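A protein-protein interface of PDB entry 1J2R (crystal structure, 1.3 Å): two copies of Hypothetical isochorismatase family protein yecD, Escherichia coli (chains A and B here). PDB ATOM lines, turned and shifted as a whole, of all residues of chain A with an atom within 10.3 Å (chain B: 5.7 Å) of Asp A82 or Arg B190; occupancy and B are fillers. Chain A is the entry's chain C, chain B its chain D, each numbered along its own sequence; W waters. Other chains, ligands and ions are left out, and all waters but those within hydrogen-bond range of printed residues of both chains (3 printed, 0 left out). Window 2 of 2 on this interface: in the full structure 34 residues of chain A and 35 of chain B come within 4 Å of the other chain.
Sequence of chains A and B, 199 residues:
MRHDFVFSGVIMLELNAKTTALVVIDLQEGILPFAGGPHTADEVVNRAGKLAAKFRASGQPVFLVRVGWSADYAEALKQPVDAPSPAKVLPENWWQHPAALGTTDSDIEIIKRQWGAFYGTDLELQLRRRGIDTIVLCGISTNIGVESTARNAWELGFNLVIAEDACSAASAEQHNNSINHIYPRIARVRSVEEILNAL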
ATOM      1  N   LYS A  78      16.543  22.521   3.270  1.00  0.00           N
ATOM      2  CA  LYS A  78      17.567  22.810   4.267  1.00  0.00           C
ATOM      3  C   LYS A  78      18.347  21.597   4.762  1.00  0.00           C
ATOM      4  O   LYS A  78      19.086  21.708   5.731  1.00  0.00           O
ATOM      5  CB  LYS A  78      16.917  23.511   5.462  1.00  0.00           C
ATOM      6  CG  LYS A  78      17.310  24.942   5.592  1.00  0.00           C
ATOM      7  CD  LYS A  78      16.340  25.836   4.886  1.00  0.00           C
ATOM      8  CE  LYS A  78      15.253  26.342   5.827  1.00  0.00           C
ATOM      9  NZ  LYS A  78      14.023  26.661   5.070  1.00  0.00           N
ATOM     10  N   GLN A  79      18.215  20.446   4.111  1.00  0.00           N
ATOM     11  CA  GLN A  79      18.953  19.257   4.542  1.00  0.00           C
ATOM     12  C   GLN A  79      20.448  19.519   4.454  1.00  0.00           C
ATOM     13  O   GLN A  79      20.896  20.258   3.575  1.00  0.00           O
ATOM     14  CB  GLN A  79      18.669  18.042   3.655  1.00  0.00           C
ATOM     15  CG  GLN A  79      17.229  17.681   3.486  1.00  0.00           C
ATOM     16  CD  GLN A  79      16.692  18.153   2.158  1.00  0.00           C
ATOM     17  OE1 GLN A  79      16.225  17.337   1.330  1.00  0.00           O
ATOM     18  NE2 GLN A  79      16.805  19.454   1.916  1.00  0.00           N
ATOM     19  N   PRO A  80      21.231  18.861   5.316  1.00  0.00           N
ATOM     20  CA  PRO A  80      22.685  18.927   5.196  1.00  0.00           C
ATOM     21  C   PRO A  80      23.155  18.368   3.857  1.00  0.00           C
ATOM     22  O   PRO A  80      22.694  17.315   3.415  1.00  0.00           O
ATOM     23  CB  PRO A  80      23.196  18.070   6.369  1.00  0.00           C
ATOM     24  CG  PRO A  80      22.065  17.343   6.900  1.00  0.00           C
ATOM     25  CD  PRO A  80      20.800  18.015   6.438  1.00  0.00           C
ATOM     26  N   VAL A  81      24.018  19.132   3.201  1.00  0.00           N
ATOM     27  CA  VAL A  81      24.696  18.725   1.956  1.00  0.00           C
ATOM     28  C   VAL A  81      26.171  19.152   2.030  1.00  0.00           C
ATOM     29  O   VAL A  81      26.529  19.989   2.849  1.00  0.00           O
ATOM     30  CB  VAL A  81      24.018  19.329   0.691  1.00  0.00           C
ATOM     31  CG1 VAL A  81      22.526  18.964   0.631  1.00  0.00           C
ATOM     32  CG2 VAL A  81      24.197  20.841   0.630  1.00  0.00           C
ATOM     33  N   ASP A  82      27.027  18.612   1.172  1.00  0.00           N
ATOM     34  CA  ASP A  82      28.443  18.953   1.187  1.00  0.00           C
ATOM     35  C   ASP A  82      28.701  20.361   0.650  1.00  0.00           C
ATOM     36  O   ASP A  82      29.667  21.017   1.080  1.00  0.00           O
ATOM     37  CB  ASP A  82      29.262  17.970   0.361  1.00  0.00           C
ATOM     38  CG  ASP A  82      29.358  16.609   0.969  1.00  0.00           C
ATOM     39  OD1 ASP A  82      29.176  16.445   2.203  1.00  0.00           O
ATOM     40  OD2 ASP A  82      29.596  15.612   0.222  1.00  0.00           O
ATOM     41  N   ALA A  83      27.875  20.826  -0.279  1.00  0.00           N
ATOM     42  CA  ALA A  83      28.106  22.097  -0.988  1.00  0.00           C
ATOM     43  C   ALA A  83      26.825  22.943  -1.003  1.00  0.00           C
ATOM     44  O   ALA A  83      26.177  23.100  -2.039  1.00  0.00           O
ATOM     45  CB  ALA A  83      28.581  21.834  -2.405  1.00  0.00           C
ATOM     46  N   PRO A  84      26.451  23.482   0.152  1.00  0.00           N
ATOM     47  CA  PRO A  84      25.206  24.248   0.276  1.00  0.00           C
ATOM     48  C   PRO A  84      25.326  25.609  -0.399  1.00  0.00           C
ATOM     49  O   PRO A  84      26.426  26.143  -0.498  1.00  0.00           O
ATOM     50  CB  PRO A  84      25.058  24.416   1.791  1.00  0.00           C
ATOM     51  CG  PRO A  84      26.432  24.367   2.312  1.00  0.00           C
ATOM     52  CD  PRO A  84      27.191  23.409   1.423  1.00  0.00           C
ATOM     53  N   SER A  85      24.217  26.128  -0.915  1.00  0.00           N
ATOM     54  CA  SER A  85      24.189  27.480  -1.456  1.00  0.00           C
ATOM     55  C   SER A  85      23.941  28.445  -0.287  1.00  0.00           C
ATOM     56  O   SER A  85      23.148  28.152   0.600  1.00  0.00           O
ATOM     57  CB  SER A  85      23.087  27.619  -2.510  1.00  0.00           C
ATOM     58  OG  SER A  85      23.336  26.819  -3.654  1.00  0.00           O
ATOM     59  N   PRO A  86      24.617  29.591  -0.270  1.00  0.00           N
ATOM     60  CA  PRO A  86      24.441  30.556   0.823  1.00  0.00           C
ATOM     61  C   PRO A  86      23.069  31.229   0.754  1.00  0.00           C
ATOM     62  O   PRO A  86      22.598  31.512  -0.340  1.00  0.00           O
ATOM     63  CB  PRO A  86      25.572  31.564   0.583  1.00  0.00           C
ATOM     64  CG  PRO A  86      25.873  31.477  -0.852  1.00  0.00           C
ATOM     65  CD  PRO A  86      25.593  30.060  -1.269  1.00  0.00           C
ATOM     66  N   LEU B  13      31.188  11.947  10.207  1.00  0.00           N
ATOM     67  CA  LEU B  13      29.837  11.839   9.641  1.00  0.00           C
ATOM     68  C   LEU B  13      28.868  11.545  10.766  1.00  0.00           C
ATOM     69  O   LEU B  13      29.116  10.650  11.565  1.00  0.00           O
ATOM     70  CB  LEU B  13      29.748  10.729   8.582  1.00  0.00           C
ATOM     71  CG  LEU B  13      28.363  10.375   8.029  1.00  0.00           C
ATOM     72  CD1 LEU B  13      27.756  11.515   7.220  1.00  0.00           C
ATOM     73  CD2 LEU B  13      28.426   9.095   7.180  1.00  0.00           C
ATOM     74  N   VAL B 161      22.605  10.605   1.873  1.00  0.00           N
ATOM     75  CA  VAL B 161      24.005  10.239   1.967  1.00  0.00           C
ATOM     76  C   VAL B 161      24.287   9.276   0.808  1.00  0.00           C
ATOM     77  O   VAL B 161      23.571   8.292   0.648  1.00  0.00           O
ATOM     78  CB  VAL B 161      24.319   9.568   3.309  1.00  0.00           C
ATOM     79  CG1 VAL B 161      25.754   9.094   3.342  1.00  0.00           C
ATOM     80  CG2 VAL B 161      24.053  10.549   4.452  1.00  0.00           C
ATOM     81  N   ILE B 162      25.267   9.602  -0.040  1.00  0.00           N
ATOM     82  CA  ILE B 162      25.631   8.743  -1.164  1.00  0.00           C
ATOM     83  C   ILE B 162      26.849   7.929  -0.757  1.00  0.00           C
ATOM     84  O   ILE B 162      27.863   8.498  -0.370  1.00  0.00           O
ATOM     85  CB  ILE B 162      25.987   9.566  -2.419  1.00  0.00           C
ATOM     86  CG1 ILE B 162      24.886  10.558  -2.801  1.00  0.00           C
ATOM     87  CG2 ILE B 162      26.340   8.638  -3.552  1.00  0.00           C
ATOM     88  CD1 ILE B 162      23.533   9.975  -2.974  1.00  0.00           C
ATOM     89  N   ALA B 163      26.770   6.610  -0.879  1.00  0.00           N
ATOM     90  CA  ALA B 163      27.905   5.723  -0.605  1.00  0.00           C
ATOM     91  C   ALA B 163      28.680   5.625  -1.918  1.00  0.00           C
ATOM     92  O   ALA B 163      28.368   4.798  -2.781  1.00  0.00           O
ATOM     93  CB  ALA B 163      27.397   4.361  -0.160  1.00  0.00           C
ATOM     94  N   GLU B 164      29.670   6.489  -2.089  1.00  0.00           N
ATOM     95  CA  GLU B 164      30.333   6.683  -3.378  1.00  0.00           C
ATOM     96  C   GLU B 164      30.916   5.405  -3.951  1.00  0.00           C
ATOM     97  O   GLU B 164      30.815   5.141  -5.149  1.00  0.00           O
ATOM     98  CB  GLU B 164      31.420   7.750  -3.266  1.00  0.00           C
ATOM     99  CG  GLU B 164      32.145   8.043  -4.587  1.00  0.00           C
ATOM    100  CD  GLU B 164      33.289   7.097  -4.925  1.00  0.00           C
ATOM    101  OE1 GLU B 164      33.946   6.531  -4.010  1.00  0.00           O
ATOM    102  OE2 GLU B 164      33.511   6.912  -6.151  1.00  0.00           O
ATOM    103  N   ASP B 165      31.541   4.612  -3.094  1.00  0.00           N
ATOM    104  CA  ASP B 165      32.239   3.412  -3.552  1.00  0.00           C
ATOM    105  C   ASP B 165      31.338   2.179  -3.590  1.00  0.00           C
ATOM    106  O   ASP B 165      31.776   1.074  -3.883  1.00  0.00           O
ATOM    107  CB  ASP B 165      33.563   3.201  -2.804  1.00  0.00           C
ATOM    108  CG  ASP B 165      33.412   3.094  -1.323  1.00  0.00           C
ATOM    109  OD1 ASP B 165      32.461   3.610  -0.727  1.00  0.00           O
ATOM    110  OD2 ASP B 165      34.269   2.496  -0.636  1.00  0.00           O
ATOM    111  N   TYR B 183      25.833  15.479  -6.800  1.00  0.00           N
ATOM    112  CA  TYR B 183      25.596  14.983  -5.468  1.00  0.00           C
ATOM    113  C   TYR B 183      26.031  15.915  -4.334  1.00  0.00           C
ATOM    114  O   TYR B 183      25.324  15.959  -3.340  1.00  0.00           O
ATOM    115  CB  TYR B 183      26.186  13.596  -5.294  1.00  0.00           C
ATOM    116  CG  TYR B 183      25.448  12.515  -6.041  1.00  0.00           C
ATOM    117  CD1 TYR B 183      24.110  12.295  -5.824  1.00  0.00           C
ATOM    118  CD2 TYR B 183      26.086  11.686  -6.946  1.00  0.00           C
ATOM    119  CE1 TYR B 183      23.445  11.283  -6.473  1.00  0.00           C
ATOM    120  CE2 TYR B 183      25.424  10.659  -7.593  1.00  0.00           C
ATOM    121  CZ  TYR B 183      24.082  10.479  -7.368  1.00  0.00           C
ATOM    122  OH  TYR B 183      23.372   9.491  -7.995  1.00  0.00           O
ATOM    123  N   PRO B 184      27.153  16.639  -4.418  1.00  0.00           N
ATOM    124  CA  PRO B 184      27.512  17.513  -3.289  1.00  0.00           C
ATOM    125  C   PRO B 184      26.448  18.558  -2.958  1.00  0.00           C
ATOM    126  O   PRO B 184      26.398  19.000  -1.818  1.00  0.00           O
ATOM    127  CB  PRO B 184      28.824  18.157  -3.744  1.00  0.00           C
ATOM    128  CG  PRO B 184      29.394  17.201  -4.744  1.00  0.00           C
ATOM    129  CD  PRO B 184      28.174  16.689  -5.490  1.00  0.00           C
ATOM    130  N   ARG B 185      25.642  18.965  -3.935  1.00  0.00           N
ATOM    131  CA  ARG B 185      24.616  19.989  -3.740  1.00  0.00           C
ATOM    132  C   ARG B 185      23.344  19.438  -3.110  1.00  0.00           C
ATOM    133  O   ARG B 185      22.530  20.210  -2.598  1.00  0.00           O
ATOM    134  CB  ARG B 185      24.293  20.693  -5.062  1.00  0.00           C
ATOM    135  CG  ARG B 185      25.474  21.459  -5.651  1.00  0.00           C
ATOM    136  CD  ARG B 185      25.127  22.381  -6.794  1.00  0.00           C
ATOM    137  NE  ARG B 185      24.084  23.346  -6.453  1.00  0.00           N
ATOM    138  CZ  ARG B 185      23.429  24.105  -7.337  1.00  0.00           C
ATOM    139  NH1 ARG B 185      22.482  24.936  -6.924  1.00  0.00           N
ATOM    140  NH2 ARG B 185      23.713  24.035  -8.627  1.00  0.00           N
ATOM    141  N   ALA B 187      23.401  16.166  -1.197  1.00  0.00           N
ATOM    142  CA  ALA B 187      23.763  15.016  -0.380  1.00  0.00           C
ATOM    143  C   ALA B 187      25.082  15.263   0.322  1.00  0.00           C
ATOM    144  O   ALA B 187      25.854  16.158  -0.038  1.00  0.00           O
ATOM    145  CB  ALA B 187      23.882  13.767  -1.239  1.00  0.00           C
ATOM    146  N   ARG B 188      25.337  14.433   1.323  1.00  0.00           N
ATOM    147  CA  ARG B 188      26.686  14.194   1.824  1.00  0.00           C
ATOM    148  C   ARG B 188      27.222  12.950   1.128  1.00  0.00           C
ATOM    149  O   ARG B 188      26.603  11.895   1.166  1.00  0.00           O
ATOM    150  CB  ARG B 188      26.667  13.991   3.330  1.00  0.00           C
ATOM    151  CG  ARG B 188      26.393  15.271   4.101  1.00  0.00           C
ATOM    152  CD  ARG B 188      26.105  15.056   5.578  1.00  0.00           C
ATOM    153  NE  ARG B 188      24.813  14.401   5.766  1.00  0.00           N
ATOM    154  CZ  ARG B 188      24.366  13.885   6.899  1.00  0.00           C
ATOM    155  NH1 ARG B 188      25.108  13.914   7.997  1.00  0.00           N
ATOM    156  NH2 ARG B 188      23.172  13.330   6.926  1.00  0.00           N
ATOM    157  N   VAL B 189      28.375  13.096   0.477  1.00  0.00           N
ATOM    158  CA  VAL B 189      29.016  12.014  -0.267  1.00  0.00           C
ATOM    159  C   VAL B 189      30.109  11.431   0.618  1.00  0.00           C
ATOM    160  O   VAL B 189      31.005  12.168   1.060  1.00  0.00           O
ATOM    161  CB  VAL B 189      29.588  12.520  -1.598  1.00  0.00           C
ATOM    162  CG1 VAL B 189      30.207  11.364  -2.368  1.00  0.00           C
ATOM    163  CG2 VAL B 189      28.494  13.192  -2.410  1.00  0.00           C
ATOM    164  N   ARG B 190      30.026  10.141   0.892  1.00  0.00           N
ATOM    165  CA  ARG B 190      30.971   9.502   1.804  1.00  0.00           C
ATOM    166  C   ARG B 190      31.297   8.100   1.330  1.00  0.00           C
ATOM    167  O   ARG B 190      30.624   7.521   0.484  1.00  0.00           O
ATOM    168  CB  ARG B 190      30.357   9.410   3.202  1.00  0.00           C
ATOM    169  CG  ARG B 190      30.114  10.766   3.861  1.00  0.00           C
ATOM    170  CD  ARG B 190      31.361  11.545   4.219  1.00  0.00           C
ATOM    171  NE  ARG B 190      31.035  12.744   4.999  1.00  0.00           N
ATOM    172  CZ  ARG B 190      30.541  13.875   4.492  1.00  0.00           C
ATOM    173  NH1 ARG B 190      30.341  14.023   3.195  1.00  0.00           N
ATOM    174  NH2 ARG B 190      30.244  14.895   5.290  1.00  0.00           N
ATOM    175  N   SER B 191      32.355   7.524   1.891  1.00  0.00           N
ATOM    176  CA  SER B 191      32.688   6.139   1.594  1.00  0.00           C
ATOM    177  C   SER B 191      31.875   5.171   2.440  1.00  0.00           C
ATOM    178  O   SER B 191      31.351   5.516   3.507  1.00  0.00           O
ATOM    179  CB  SER B 191      34.164   5.895   1.859  1.00  0.00           C
ATOM    180  OG  SER B 191      34.404   5.941   3.259  1.00  0.00           O
ATOM    181  N   VAL B 192      31.819   3.930   1.993  1.00  0.00           N
ATOM    182  CA  VAL B 192      31.166   2.887   2.757  1.00  0.00           C
ATOM    183  C   VAL B 192      31.794   2.755   4.160  1.00  0.00           C
ATOM    184  O   VAL B 192      31.076   2.605   5.142  1.00  0.00           O
ATOM    185  CB  VAL B 192      31.221   1.558   1.991  1.00  0.00           C
ATOM    186  CG1 VAL B 192      30.860   0.384   2.883  1.00  0.00           C
ATOM    187  CG2 VAL B 192      30.299   1.617   0.775  1.00  0.00           C
ATOM    188  N   GLU B 194      33.240   5.089   5.953  1.00  0.00           N
ATOM    189  CA  GLU B 194      32.791   6.223   6.751  1.00  0.00           C
ATOM    190  C   GLU B 194      31.351   6.035   7.225  1.00  0.00           C
ATOM    191  O   GLU B 194      31.015   6.353   8.368  1.00  0.00           O
ATOM    192  CB  GLU B 194      32.917   7.534   5.985  1.00  0.00           C
ATOM    193  CG  GLU B 194      34.353   8.010   5.872  1.00  0.00           C
ATOM    194  CD  GLU B 194      34.560   9.067   4.796  1.00  0.00           C
ATOM    195  OE1 GLU B 194      33.755   9.196   3.845  1.00  0.00           O
ATOM    196  OE2 GLU B 194      35.566   9.784   4.885  1.00  0.00           O
ATOM    197  N   ILE B 195      30.493   5.517   6.351  1.00  0.00           N
ATOM    198  CA  ILE B 195      29.105   5.299   6.690  1.00  0.00           C
ATOM    199  C   ILE B 195      28.983   4.194   7.751  1.00  0.00           C
ATOM    200  O   ILE B 195      28.248   4.351   8.730  1.00  0.00           O
ATOM    201  CB  ILE B 195      28.272   4.977   5.412  1.00  0.00           C
ATOM    202  CG1 ILE B 195      28.229   6.195   4.485  1.00  0.00           C
ATOM    203  CG2 ILE B 195      26.855   4.544   5.777  1.00  0.00           C
ATOM    204  CD1 ILE B 195      27.944   5.890   3.046  1.00  0.00           C
HETATM  205  O   HOH W   1      22.505  14.559   4.108  1.00  0.00           O
HETATM  206  O   HOH W   2      24.138  24.123  -3.551  1.00  0.00           O
HETATM  207  O   HOH W   3      29.342  17.636   4.590  1.00  0.00           O
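The backbone NH (N) of Ile B162 lies within hydrogen-bond range of the backbone carbonyl oxygen (O) of Arg B188, at 2.9 Å.
O of Ile B162 sits at hydrogen-bond distance from N of Arg B190 (3.0 Å).
O of Arg B190 is in hydrogen-bond range of N of Glu B164 (2.9 Å).
No position is printed for both chains.
Val A81 touches Pro B184.
O of Arg B185 touches CG1 of Val A81 (3.5 Å).
Ala B187 touches Val A81.
OD1 of Asp A82 touches CA of Arg B188 (3.4 Å).
Arg B185 touches Ala A83.
Ser A85 touches Arg B185.
Water W3 bridges OD1 of Asp A82 (2.7 Å) and NH2 of Arg B190 (3.0 Å).
Water W2 lies within hydrogen-bond range of the backbone carbonyl oxygen (O) of Ala A83 (2.7 Å), the side-chain hydroxyl (OG) of Ser A85 (2.8 Å) and the guanidinium group (NE) of Arg B185 (3.0 Å).
Water W1 bridges NE of Arg B188 (2.8 Å) and O of Pro A80 (2.8 Å).
Of the printed residues of chain B, Val A81 touches Pro B184, Arg B185 and Ala B187.
Of chain B, only Pro B184 (3.1 Å), Ala B187 (3.0 Å), Arg B188 (3.4 Å), Val B189 (2.8 Å) and Arg B190 (2.9 Å) come within 4 Å of Asp A82.
Printed residues of chain B within 4 Å of Ala A83: Pro B184 and Arg B185.
Printed residues of chain B within 4 Å of Ser A85: Arg B185 (3.9 Å).
No residue of chain A comes within 4 Å of Ala B163.
Printed residues of chain A within 4 Å of Arg B185: Val A81, Ala A83 and Ser A85.
Of chain A, only Val A81 (3.5 Å) and Asp A82 (3.0 Å) come within 4 Å of Ala B187.
Of the printed residues of chain A, Arg B188 touches Asp A82 (3.4 Å).
Of chain A, only Asp A82 comes within 4 Å of Val B189.
Arg B190 touches just one residue of chain A: Asp A82 (2.9 Å).
No residue of chain A comes within 4 Å of Ser B191.
Val B192 touches none of the printed residues of chain A.
No residue of chain A comes within 4 Å of Glu B194.
The nearest residue of chain B that does not touch Asp A82 is Arg B185 (5.3 Å).
The nearest residue of chain A that does not touch Arg B190 is Val A81 (6.7 Å).
O of Pro B184 is in hydrogen-bond range of N of Asp A82, at 3.1 Å.
N of Asp A82 lies within hydrogen-bond range of O of Ala B187 (3.0 Å).
N of Val B189 sits at hydrogen-bond distance from OD2 of Asp A82 (2.8 Å).
OD1 of Asp A82 lies within salt-bridge range of NH1 of Arg B190, at 2.9 Å.
The backbone carbonyl oxygen (O) of Pro B184 lies within hydrogen-bond range of the backbone NH (N) of Ala A83, 2.8 Å away.
Of the 17 printed residues of chain B, 6 touch a printed residue of chain A.
Hydrophobic or aromatic side chains of chain B within 4 Å of the printed part of chain A: Pro B184 and Val B189.
Along chain A the printed residues that touch a printed residue of chain B span positions 81 to 85.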
